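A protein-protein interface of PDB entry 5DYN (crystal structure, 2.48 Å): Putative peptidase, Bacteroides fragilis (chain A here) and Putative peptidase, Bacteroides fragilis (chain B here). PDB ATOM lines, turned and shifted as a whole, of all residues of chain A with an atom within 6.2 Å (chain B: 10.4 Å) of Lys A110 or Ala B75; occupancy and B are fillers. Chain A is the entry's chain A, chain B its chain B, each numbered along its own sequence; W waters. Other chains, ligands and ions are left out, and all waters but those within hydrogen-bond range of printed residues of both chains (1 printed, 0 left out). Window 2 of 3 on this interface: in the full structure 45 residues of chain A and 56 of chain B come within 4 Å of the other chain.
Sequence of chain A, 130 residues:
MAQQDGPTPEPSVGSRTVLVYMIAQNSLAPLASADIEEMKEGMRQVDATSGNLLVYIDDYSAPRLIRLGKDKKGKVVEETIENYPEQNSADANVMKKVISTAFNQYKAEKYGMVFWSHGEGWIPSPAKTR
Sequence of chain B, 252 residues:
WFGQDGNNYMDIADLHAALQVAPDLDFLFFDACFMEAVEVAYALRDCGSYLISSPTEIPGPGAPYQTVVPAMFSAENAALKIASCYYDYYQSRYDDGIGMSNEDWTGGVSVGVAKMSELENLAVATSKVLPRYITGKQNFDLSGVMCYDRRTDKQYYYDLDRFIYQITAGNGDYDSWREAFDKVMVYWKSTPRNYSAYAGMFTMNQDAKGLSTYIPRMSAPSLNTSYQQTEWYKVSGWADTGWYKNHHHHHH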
ATOM      1  N   GLY A  14      16.784 -21.224   5.355  1.00  0.00           N
ATOM      2  CA  GLY A  14      17.645 -20.059   5.223  1.00  0.00           C
ATOM      3  C   GLY A  14      17.696 -19.434   3.838  1.00  0.00           C
ATOM      4  O   GLY A  14      18.436 -18.477   3.606  1.00  0.00           O
ATOM      5  N   SER A  15      16.902 -19.969   2.919  1.00  0.00           N
ATOM      6  CA  SER A  15      16.908 -19.523   1.530  1.00  0.00           C
ATOM      7  C   SER A  15      16.256 -18.151   1.340  1.00  0.00           C
ATOM      8  O   SER A  15      15.380 -17.753   2.110  1.00  0.00           O
ATOM      9  CB  SER A  15      16.204 -20.562   0.659  1.00  0.00           C
ATOM     10  OG  SER A  15      14.874 -20.774   1.102  1.00  0.00           O
ATOM     11  N   ARG A  16      16.690 -17.429   0.310  1.00  0.00           N
ATOM     12  CA  ARG A  16      16.083 -16.143  -0.027  1.00  0.00           C
ATOM     13  C   ARG A  16      16.027 -15.928  -1.536  1.00  0.00           C
ATOM     14  O   ARG A  16      16.957 -16.286  -2.257  1.00  0.00           O
ATOM     15  CB  ARG A  16      16.847 -14.993   0.630  1.00  0.00           C
ATOM     16  CG  ARG A  16      16.129 -13.657   0.520  1.00  0.00           C
ATOM     17  CD  ARG A  16      17.084 -12.491   0.683  1.00  0.00           C
ATOM     18  NE  ARG A  16      17.700 -12.450   2.007  1.00  0.00           N
ATOM     19  CZ  ARG A  16      17.220 -11.761   3.039  1.00  0.00           C
ATOM     20  NH1 ARG A  16      16.106 -11.051   2.909  1.00  0.00           N
ATOM     21  NH2 ARG A  16      17.854 -11.783   4.204  1.00  0.00           N
ATOM     22  N   THR A  17      14.933 -15.338  -2.007  1.00  0.00           N
ATOM     23  CA  THR A  17      14.786 -15.000  -3.420  1.00  0.00           C
ATOM     24  C   THR A  17      14.640 -13.493  -3.607  1.00  0.00           C
ATOM     25  O   THR A  17      13.784 -12.861  -2.987  1.00  0.00           O
ATOM     26  CB  THR A  17      13.571 -15.706  -4.053  1.00  0.00           C
ATOM     27  OG1 THR A  17      13.766 -17.126  -4.017  1.00  0.00           O
ATOM     28  CG2 THR A  17      13.387 -15.262  -5.498  1.00  0.00           C
ATOM     29  N   VAL A  18      15.481 -12.920  -4.462  1.00  0.00           N
ATOM     30  CA  VAL A  18      15.413 -11.493  -4.752  1.00  0.00           C
ATOM     31  C   VAL A  18      15.228 -11.253  -6.246  1.00  0.00           C
ATOM     32  O   VAL A  18      16.020 -11.717  -7.063  1.00  0.00           O
ATOM     33  CB  VAL A  18      16.679 -10.755  -4.273  1.00  0.00           C
ATOM     34  CG1 VAL A  18      16.609  -9.278  -4.647  1.00  0.00           C
ATOM     35  CG2 VAL A  18      16.862 -10.925  -2.771  1.00  0.00           C
ATOM     36  N   LYS A 107      10.366 -20.189  -4.696  1.00  0.00           N
ATOM     37  CA  LYS A 107       9.940 -19.973  -3.321  1.00  0.00           C
ATOM     38  C   LYS A 107      11.141 -20.058  -2.388  1.00  0.00           C
ATOM     39  O   LYS A 107      12.065 -20.836  -2.620  1.00  0.00           O
ATOM     40  CB  LYS A 107       8.872 -20.993  -2.911  1.00  0.00           C
ATOM     41  CG  LYS A 107       7.475 -20.681  -3.427  1.00  0.00           C
ATOM     42  CD  LYS A 107       6.979 -21.744  -4.395  1.00  0.00           C
ATOM     43  CE  LYS A 107       5.595 -21.403  -4.928  1.00  0.00           C
ATOM     44  NZ  LYS A 107       5.130 -22.377  -5.955  1.00  0.00           N
ATOM     45  N   ALA A 108      11.130 -19.246  -1.339  1.00  0.00           N
ATOM     46  CA  ALA A 108      12.217 -19.255  -0.370  1.00  0.00           C
ATOM     47  C   ALA A 108      11.713 -18.894   1.021  1.00  0.00           C
ATOM     48  O   ALA A 108      10.523 -18.647   1.218  1.00  0.00           O
ATOM     49  CB  ALA A 108      13.314 -18.301  -0.800  1.00  0.00           C
ATOM     50  N   GLU A 109      12.628 -18.874   1.984  1.00  0.00           N
ATOM     51  CA  GLU A 109      12.293 -18.491   3.347  1.00  0.00           C
ATOM     52  C   GLU A 109      12.020 -16.995   3.424  1.00  0.00           C
ATOM     53  O   GLU A 109      11.075 -16.561   4.078  1.00  0.00           O
ATOM     54  CB  GLU A 109      13.421 -18.875   4.304  1.00  0.00           C
ATOM     55  CG  GLU A 109      13.242 -18.371   5.719  1.00  0.00           C
ATOM     56  CD  GLU A 109      14.347 -18.848   6.637  1.00  0.00           C
ATOM     57  OE1 GLU A 109      14.572 -20.075   6.705  1.00  0.00           O
ATOM     58  OE2 GLU A 109      14.993 -17.999   7.287  1.00  0.00           O
ATOM     59  N   LYS A 110      12.856 -16.212   2.748  1.00  0.00           N
ATOM     60  CA  LYS A 110      12.689 -14.764   2.712  1.00  0.00           C
ATOM     61  C   LYS A 110      12.653 -14.246   1.276  1.00  0.00           C
ATOM     62  O   LYS A 110      13.087 -14.924   0.344  1.00  0.00           O
ATOM     63  CB  LYS A 110      13.809 -14.075   3.497  1.00  0.00           C
ATOM     64  CG  LYS A 110      13.947 -14.572   4.924  1.00  0.00           C
ATOM     65  CD  LYS A 110      14.620 -13.552   5.823  1.00  0.00           C
ATOM     66  CE  LYS A 110      14.620 -14.036   7.264  1.00  0.00           C
ATOM     67  NZ  LYS A 110      14.915 -12.947   8.230  1.00  0.00           N
ATOM     68  N   TYR A 111      12.128 -13.037   1.107  1.00  0.00           N
ATOM     69  CA  TYR A 111      12.033 -12.421  -0.209  1.00  0.00           C
ATOM     70  C   TYR A 111      12.482 -10.967  -0.177  1.00  0.00           C
ATOM     71  O   TYR A 111      12.530 -10.339   0.880  1.00  0.00           O
ATOM     72  CB  TYR A 111      10.603 -12.507  -0.741  1.00  0.00           C
ATOM     73  CG  TYR A 111      10.079 -13.917  -0.861  1.00  0.00           C
ATOM     74  CD1 TYR A 111      10.409 -14.711  -1.951  1.00  0.00           C
ATOM     75  CD2 TYR A 111       9.253 -14.456   0.116  1.00  0.00           C
ATOM     76  CE1 TYR A 111       9.928 -16.003  -2.067  1.00  0.00           C
ATOM     77  CE2 TYR A 111       8.768 -15.746   0.011  1.00  0.00           C
ATOM     78  CZ  TYR A 111       9.108 -16.515  -1.082  1.00  0.00           C
ATOM     79  OH  TYR A 111       8.629 -17.800  -1.189  1.00  0.00           O
ATOM     80  N   GLY A 112      12.809 -10.441  -1.351  1.00  0.00           N
ATOM     81  CA  GLY A 112      13.147  -9.042  -1.502  1.00  0.00           C
ATOM     82  C   GLY A 112      12.948  -8.639  -2.947  1.00  0.00           C
ATOM     83  O   GLY A 112      12.951  -9.493  -3.839  1.00  0.00           O
ATOM     84  N   ALA B  22       2.972 -10.332  -5.388  1.00  0.00           N
ATOM     85  CA  ALA B  22       4.257 -10.609  -4.765  1.00  0.00           C
ATOM     86  C   ALA B  22       4.047 -11.160  -3.367  1.00  0.00           C
ATOM     87  O   ALA B  22       3.080 -10.802  -2.700  1.00  0.00           O
ATOM     88  CB  ALA B  22       5.116  -9.349  -4.718  1.00  0.00           C
ATOM     89  N   PRO B  23       4.953 -12.041  -2.918  1.00  0.00           N
ATOM     90  CA  PRO B  23       4.931 -12.441  -1.509  1.00  0.00           C
ATOM     91  C   PRO B  23       5.346 -11.258  -0.649  1.00  0.00           C
ATOM     92  O   PRO B  23       5.869 -10.283  -1.192  1.00  0.00           O
ATOM     93  CB  PRO B  23       5.962 -13.569  -1.448  1.00  0.00           C
ATOM     94  CG  PRO B  23       6.903 -13.274  -2.564  1.00  0.00           C
ATOM     95  CD  PRO B  23       6.061 -12.670  -3.657  1.00  0.00           C
ATOM     96  N   ASP B  24       5.118 -11.321   0.657  1.00  0.00           N
ATOM     97  CA  ASP B  24       5.537 -10.222   1.513  1.00  0.00           C
ATOM     98  C   ASP B  24       7.053 -10.105   1.469  1.00  0.00           C
ATOM     99  O   ASP B  24       7.768 -11.084   1.680  1.00  0.00           O
ATOM    100  CB  ASP B  24       5.055 -10.409   2.947  1.00  0.00           C
ATOM    101  CG  ASP B  24       5.433  -9.242   3.837  1.00  0.00           C
ATOM    102  OD1 ASP B  24       4.870  -8.142   3.642  1.00  0.00           O
ATOM    103  OD2 ASP B  24       6.297  -9.416   4.723  1.00  0.00           O
ATOM    104  N   LEU B  25       7.533  -8.902   1.186  1.00  0.00           N
ATOM    105  CA  LEU B  25       8.954  -8.676   0.974  1.00  0.00           C
ATOM    106  C   LEU B  25       9.655  -8.214   2.244  1.00  0.00           C
ATOM    107  O   LEU B  25       9.080  -7.487   3.050  1.00  0.00           O
ATOM    108  CB  LEU B  25       9.152  -7.650  -0.142  1.00  0.00           C
ATOM    109  CG  LEU B  25       8.445  -7.991  -1.456  1.00  0.00           C
ATOM    110  CD1 LEU B  25       8.531  -6.835  -2.434  1.00  0.00           C
ATOM    111  CD2 LEU B  25       9.037  -9.253  -2.065  1.00  0.00           C
ATOM    112  N   ASP B  26      10.897  -8.646   2.428  1.00  0.00           N
ATOM    113  CA  ASP B  26      11.701  -8.147   3.536  1.00  0.00           C
ATOM    114  C   ASP B  26      12.028  -6.678   3.297  1.00  0.00           C
ATOM    115  O   ASP B  26      11.970  -5.856   4.214  1.00  0.00           O
ATOM    116  CB  ASP B  26      12.987  -8.964   3.695  1.00  0.00           C
ATOM    117  CG  ASP B  26      13.959  -8.338   4.685  1.00  0.00           C
ATOM    118  OD1 ASP B  26      13.500  -7.736   5.679  1.00  0.00           O
ATOM    119  OD2 ASP B  26      15.184  -8.448   4.470  1.00  0.00           O
ATOM    120  N   PHE B  27      12.363  -6.356   2.053  1.00  0.00           N
ATOM    121  CA  PHE B  27      12.730  -4.996   1.691  1.00  0.00           C
ATOM    122  C   PHE B  27      12.231  -4.633   0.299  1.00  0.00           C
ATOM    123  O   PHE B  27      12.131  -5.490  -0.580  1.00  0.00           O
ATOM    124  CB  PHE B  27      14.251  -4.814   1.765  1.00  0.00           C
ATOM    125  CG  PHE B  27      15.029  -5.799   0.928  1.00  0.00           C
ATOM    126  CD1 PHE B  27      15.243  -5.570  -0.425  1.00  0.00           C
ATOM    127  CD2 PHE B  27      15.561  -6.945   1.498  1.00  0.00           C
ATOM    128  CE1 PHE B  27      15.958  -6.472  -1.193  1.00  0.00           C
ATOM    129  CE2 PHE B  27      16.278  -7.850   0.735  1.00  0.00           C
ATOM    130  CZ  PHE B  27      16.478  -7.613  -0.611  1.00  0.00           C
ATOM    131  N   SER B  49       8.468  -4.837   4.484  1.00  0.00           N
ATOM    132  CA  SER B  49       8.827  -4.361   5.810  1.00  0.00           C
ATOM    133  C   SER B  49       9.619  -3.056   5.757  1.00  0.00           C
ATOM    134  O   SER B  49       9.372  -2.147   6.546  1.00  0.00           O
ATOM    135  CB  SER B  49       9.626  -5.433   6.550  1.00  0.00           C
ATOM    136  OG  SER B  49       8.953  -6.678   6.497  1.00  0.00           O
ATOM    137  N   TYR B  50      10.564  -2.962   4.825  1.00  0.00           N
ATOM    138  CA  TYR B  50      11.432  -1.788   4.756  1.00  0.00           C
ATOM    139  C   TYR B  50      11.519  -1.175   3.362  1.00  0.00           C
ATOM    140  O   TYR B  50      11.614  -1.885   2.360  1.00  0.00           O
ATOM    141  CB  TYR B  50      12.833  -2.148   5.250  1.00  0.00           C
ATOM    142  CG  TYR B  50      12.845  -2.614   6.686  1.00  0.00           C
ATOM    143  CD1 TYR B  50      12.801  -1.701   7.732  1.00  0.00           C
ATOM    144  CD2 TYR B  50      12.882  -3.969   6.999  1.00  0.00           C
ATOM    145  CE1 TYR B  50      12.803  -2.121   9.047  1.00  0.00           C
ATOM    146  CE2 TYR B  50      12.884  -4.399   8.311  1.00  0.00           C
ATOM    147  CZ  TYR B  50      12.843  -3.469   9.332  1.00  0.00           C
ATOM    148  OH  TYR B  50      12.845  -3.886  10.642  1.00  0.00           O
ATOM    149  N   VAL B  69      24.573  -6.861  -3.510  1.00  0.00           N
ATOM    150  CA  VAL B  69      24.019  -8.196  -3.722  1.00  0.00           C
ATOM    151  C   VAL B  69      24.302  -9.122  -2.527  1.00  0.00           C
ATOM    152  O   VAL B  69      23.382  -9.778  -2.044  1.00  0.00           O
ATOM    153  CB  VAL B  69      24.541  -8.838  -5.037  1.00  0.00           C
ATOM    154  CG1 VAL B  69      24.426 -10.348  -4.983  1.00  0.00           C
ATOM    155  CG2 VAL B  69      23.788  -8.285  -6.236  1.00  0.00           C
ATOM    156  N   PRO B  70      25.557  -9.173  -2.030  1.00  0.00           N
ATOM    157  CA  PRO B  70      25.742  -9.962  -0.805  1.00  0.00           C
ATOM    158  C   PRO B  70      24.925  -9.434   0.376  1.00  0.00           C
ATOM    159  O   PRO B  70      24.418 -10.225   1.172  1.00  0.00           O
ATOM    160  CB  PRO B  70      27.242  -9.829  -0.523  1.00  0.00           C
ATOM    161  CG  PRO B  70      27.849  -9.556  -1.841  1.00  0.00           C
ATOM    162  CD  PRO B  70      26.852  -8.713  -2.572  1.00  0.00           C
ATOM    163  N   ALA B  71      24.800  -8.114   0.480  1.00  0.00           N
ATOM    164  CA  ALA B  71      24.004  -7.506   1.540  1.00  0.00           C
ATOM    165  C   ALA B  71      22.554  -7.971   1.467  1.00  0.00           C
ATOM    166  O   ALA B  71      21.905  -8.170   2.493  1.00  0.00           O
ATOM    167  CB  ALA B  71      24.076  -5.989   1.460  1.00  0.00           C
ATOM    168  N   MET B  72      22.055  -8.155   0.249  1.00  0.00           N
ATOM    169  CA  MET B  72      20.673  -8.575   0.047  1.00  0.00           C
ATOM    170  C   MET B  72      20.431 -10.009   0.502  1.00  0.00           C
ATOM    171  O   MET B  72      19.296 -10.391   0.773  1.00  0.00           O
ATOM    172  CB  MET B  72      20.275  -8.429  -1.423  1.00  0.00           C
ATOM    173  CG  MET B  72      20.244  -6.991  -1.908  1.00  0.00           C
ATOM    174  SD  MET B  72      19.504  -6.800  -3.538  1.00  0.00           S
ATOM    175  CE  MET B  72      20.540  -7.875  -4.519  1.00  0.00           C
ATOM    176  N   PHE B  73      21.494 -10.802   0.592  1.00  0.00           N
ATOM    177  CA  PHE B  73      21.355 -12.200   0.977  1.00  0.00           C
ATOM    178  C   PHE B  73      21.931 -12.473   2.366  1.00  0.00           C
ATOM    179  O   PHE B  73      22.379 -13.582   2.655  1.00  0.00           O
ATOM    180  CB  PHE B  73      22.018 -13.105  -0.064  1.00  0.00           C
ATOM    181  CG  PHE B  73      21.278 -13.158  -1.372  1.00  0.00           C
ATOM    182  CD1 PHE B  73      20.215 -14.028  -1.547  1.00  0.00           C
ATOM    183  CD2 PHE B  73      21.641 -12.333  -2.423  1.00  0.00           C
ATOM    184  CE1 PHE B  73      19.530 -14.077  -2.747  1.00  0.00           C
ATOM    185  CE2 PHE B  73      20.959 -12.377  -3.627  1.00  0.00           C
ATOM    186  CZ  PHE B  73      19.903 -13.248  -3.788  1.00  0.00           C
ATOM    187  N   SER B  74      21.910 -11.457   3.221  1.00  0.00           N
ATOM    188  CA  SER B  74      22.324 -11.616   4.610  1.00  0.00           C
ATOM    189  C   SER B  74      21.296 -12.436   5.375  1.00  0.00           C
ATOM    190  O   SER B  74      20.144 -12.542   4.952  1.00  0.00           O
ATOM    191  CB  SER B  74      22.511 -10.256   5.279  1.00  0.00           C
ATOM    192  OG  SER B  74      23.555  -9.523   4.663  1.00  0.00           O
ATOM    193  N   ALA B  75      21.716 -13.014   6.498  1.00  0.00           N
ATOM    194  CA  ALA B  75      20.818 -13.785   7.351  1.00  0.00           C
ATOM    195  C   ALA B  75      19.651 -12.920   7.823  1.00  0.00           C
ATOM    196  O   ALA B  75      18.487 -13.291   7.674  1.00  0.00           O
ATOM    197  CB  ALA B  75      21.576 -14.355   8.538  1.00  0.00           C
ATOM    198  N   GLU B  76      19.975 -11.762   8.388  1.00  0.00           N
ATOM    199  CA  GLU B  76      18.970 -10.781   8.779  1.00  0.00           C
ATOM    200  C   GLU B  76      19.590  -9.389   8.658  1.00  0.00           C
ATOM    201  O   GLU B  76      20.795  -9.268   8.415  1.00  0.00           O
ATOM    202  CB  GLU B  76      18.459 -11.063  10.202  1.00  0.00           C
ATOM    203  CG  GLU B  76      17.296 -10.182  10.700  1.00  0.00           C
ATOM    204  CD  GLU B  76      16.147 -10.068   9.703  1.00  0.00           C
ATOM    205  OE1 GLU B  76      15.739 -11.101   9.135  1.00  0.00           O
ATOM    206  OE2 GLU B  76      15.650  -8.941   9.490  1.00  0.00           O
ATOM    207  N   ASN B  77      18.763  -8.354   8.798  1.00  0.00           N
ATOM    208  CA  ASN B  77      19.189  -6.961   8.678  1.00  0.00           C
ATOM    209  C   ASN B  77      19.716  -6.649   7.288  1.00  0.00           C
ATOM    210  O   ASN B  77      20.601  -5.810   7.125  1.00  0.00           O
ATOM    211  CB  ASN B  77      20.246  -6.621   9.730  1.00  0.00           C
ATOM    212  CG  ASN B  77      19.679  -6.591  11.129  1.00  0.00           C
ATOM    213  OD1 ASN B  77      20.118  -7.335  12.007  1.00  0.00           O
ATOM    214  ND2 ASN B  77      18.690  -5.731  11.347  1.00  0.00           N
ATOM    215  N   ALA B  78      19.159  -7.327   6.291  1.00  0.00           N
ATOM    216  CA  ALA B  78      19.542  -7.099   4.907  1.00  0.00           C
ATOM    217  C   ALA B  78      19.303  -5.644   4.520  1.00  0.00           C
ATOM    218  O   ALA B  78      20.160  -5.018   3.899  1.00  0.00           O
ATOM    219  CB  ALA B  78      18.776  -8.032   3.983  1.00  0.00           C
ATOM    220  N   ALA B  79      18.149  -5.111   4.912  1.00  0.00           N
ATOM    221  CA  ALA B  79      17.766  -3.747   4.561  1.00  0.00           C
ATOM    222  C   ALA B  79      18.796  -2.735   5.045  1.00  0.00           C
ATOM    223  O   ALA B  79      19.190  -1.836   4.303  1.00  0.00           O
ATOM    224  CB  ALA B  79      16.395  -3.420   5.128  1.00  0.00           C
ATOM    225  N   LEU B  80      19.241  -2.894   6.287  1.00  0.00           N
ATOM    226  CA  LEU B  80      20.262  -2.011   6.844  1.00  0.00           C
ATOM    227  C   LEU B  80      21.597  -2.211   6.138  1.00  0.00           C
ATOM    228  O   LEU B  80      22.311  -1.249   5.851  1.00  0.00           O
ATOM    229  CB  LEU B  80      20.423  -2.252   8.346  1.00  0.00           C
ATOM    230  CG  LEU B  80      19.308  -1.734   9.253  1.00  0.00           C
ATOM    231  CD1 LEU B  80      19.567  -2.147  10.692  1.00  0.00           C
ATOM    232  CD2 LEU B  80      19.186  -0.223   9.140  1.00  0.00           C
ATOM    233  N   LYS B  81      21.927  -3.467   5.858  1.00  0.00           N
ATOM    234  CA  LYS B  81      23.191  -3.788   5.217  1.00  0.00           C
ATOM    235  C   LYS B  81      23.210  -3.300   3.769  1.00  0.00           C
ATOM    236  O   LYS B  81      24.245  -2.851   3.282  1.00  0.00           O
ATOM    237  CB  LYS B  81      23.456  -5.289   5.295  1.00  0.00           C
ATOM    238  CG  LYS B  81      23.834  -5.757   6.694  1.00  0.00           C
ATOM    239  CD  LYS B  81      23.710  -7.260   6.834  1.00  0.00           C
ATOM    240  CE  LYS B  81      24.197  -7.737   8.192  1.00  0.00           C
ATOM    241  NZ  LYS B  81      25.659  -7.500   8.366  1.00  0.00           N
ATOM    242  N   ILE B  82      22.064  -3.374   3.094  1.00  0.00           N
ATOM    243  CA  ILE B  82      21.928  -2.813   1.750  1.00  0.00           C
ATOM    244  C   ILE B  82      22.227  -1.315   1.757  1.00  0.00           C
ATOM    245  O   ILE B  82      23.013  -0.819   0.947  1.00  0.00           O
ATOM    246  CB  ILE B  82      20.514  -3.035   1.172  1.00  0.00           C
ATOM    247  CG1 ILE B  82      20.273  -4.518   0.881  1.00  0.00           C
ATOM    248  CG2 ILE B  82      20.323  -2.225  -0.105  1.00  0.00           C
ATOM    249  CD1 ILE B  82      18.824  -4.852   0.596  1.00  0.00           C
HETATM  250  O   HOH W   1      12.954 -10.813   9.093  1.00  0.00           O
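The side-chain carboxylate (OD2) of Asp B26 is in salt-bridge range of the guanidinium group (NH1) of Arg A16, at 3.2 Å. O of Met B72 is in hydrogen-bond range of NE of Arg A16 (2.9 Å). The backbone carbonyl oxygen (O) of Ser B74 sits at hydrogen-bond distance from the guanidinium group (NH2) of Arg A16 (2.5 Å). The backbone NH (N) of Asp B26 lies within hydrogen-bond range of the backbone carbonyl oxygen (O) of Tyr A111, 2.8 Å away. The side-chain carboxylate of Glu B76 lies close to the side-chain amino group of Lys A110 (2.2 Å).
The backbone carbonyl oxygen (O) of Ser A15 lies within hydrogen-bond range of the backbone NH (N) of Lys A110, 3.0 Å away. The backbone NH of Thr A17 lies within hydrogen-bond range of the backbone carbonyl oxygen of Lys A110. O of Thr A17 is in hydrogen-bond range of N of Gly A112. The backbone NH of Ala A108 sits at hydrogen-bond distance from the side-chain hydroxyl of Tyr A111, at 2.9 Å. The backbone carbonyl oxygen (O) of Leu B25 sits at hydrogen-bond distance from the backbone NH (N) of Ser B49 (3.1 Å). O of Ala B71 sits at hydrogen-bond distance from OG of Ser B74, at 3.0 Å.
Of the 22 printed residues of chain B, 11 touch a printed residue of chain A. Hydrophobic or aromatic side chains of chain A within 4 Å of the printed part of chain B: Val A18 and Tyr A111. Among the printed residues, 17 pairs touch across the chains. Among the printed residues, Asp or Glu carboxylates within 4 Å of a Lys or Arg side-chain nitrogen of the other chain: Arg A16 with Asp B26 and Lys A110 with Glu B76.
Water W1 lies within hydrogen-bond range of OE1 of Glu B76 (2.8 Å) and NZ of Lys A110 (3.0 Å).
Among the printed residues, merely in contact across the chains: Arg A16 with Phe B27, Arg A16 with Phe B73, Arg A16 with Ala B75, Arg A16 with Ala B78, Val A18 with Phe B27, Val A18 with Met B72, Val A18 with Phe B73, Lys A110 with Ala B75, Tyr A111 with Pro B23, Tyr A111 with Asp B24, Tyr A111 with Leu B25 and Gly A112 with Phe B27.
Of chain B, only Ala B75 (3.6 Å) and Glu B76 (2.2 Å) come within 4 Å of Lys A110. Ala B75 touches just these residues of chain A: Arg A16 and Lys A110. No residue of chain B comes within 4 Å of Thr A17. Glu A109 touches none of the printed residues of chain B. Printed residues of chain A within 4 Å of Leu B25: Tyr A111. Of the printed residues of chain A, Phe B27 touches Arg A16, Val A18 and Gly A112. Of the printed residues of chain B, Gly A112 touches Phe B27. Of the printed residues of chain A, Met B72 touches Arg A16 and Val A18. Printed residues of chain A within 4 Å of Ser B74: Arg A16. The nearest residue of chain B that does not touch Lys A110 is Asp B26 (5.2 Å). The nearest residue of chain A that does not touch Ala B75 is Glu A109 (5.9 Å). The nearest printed residue of chain A that does not touch Ser B74 is Lys A110 (5.7 Å).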
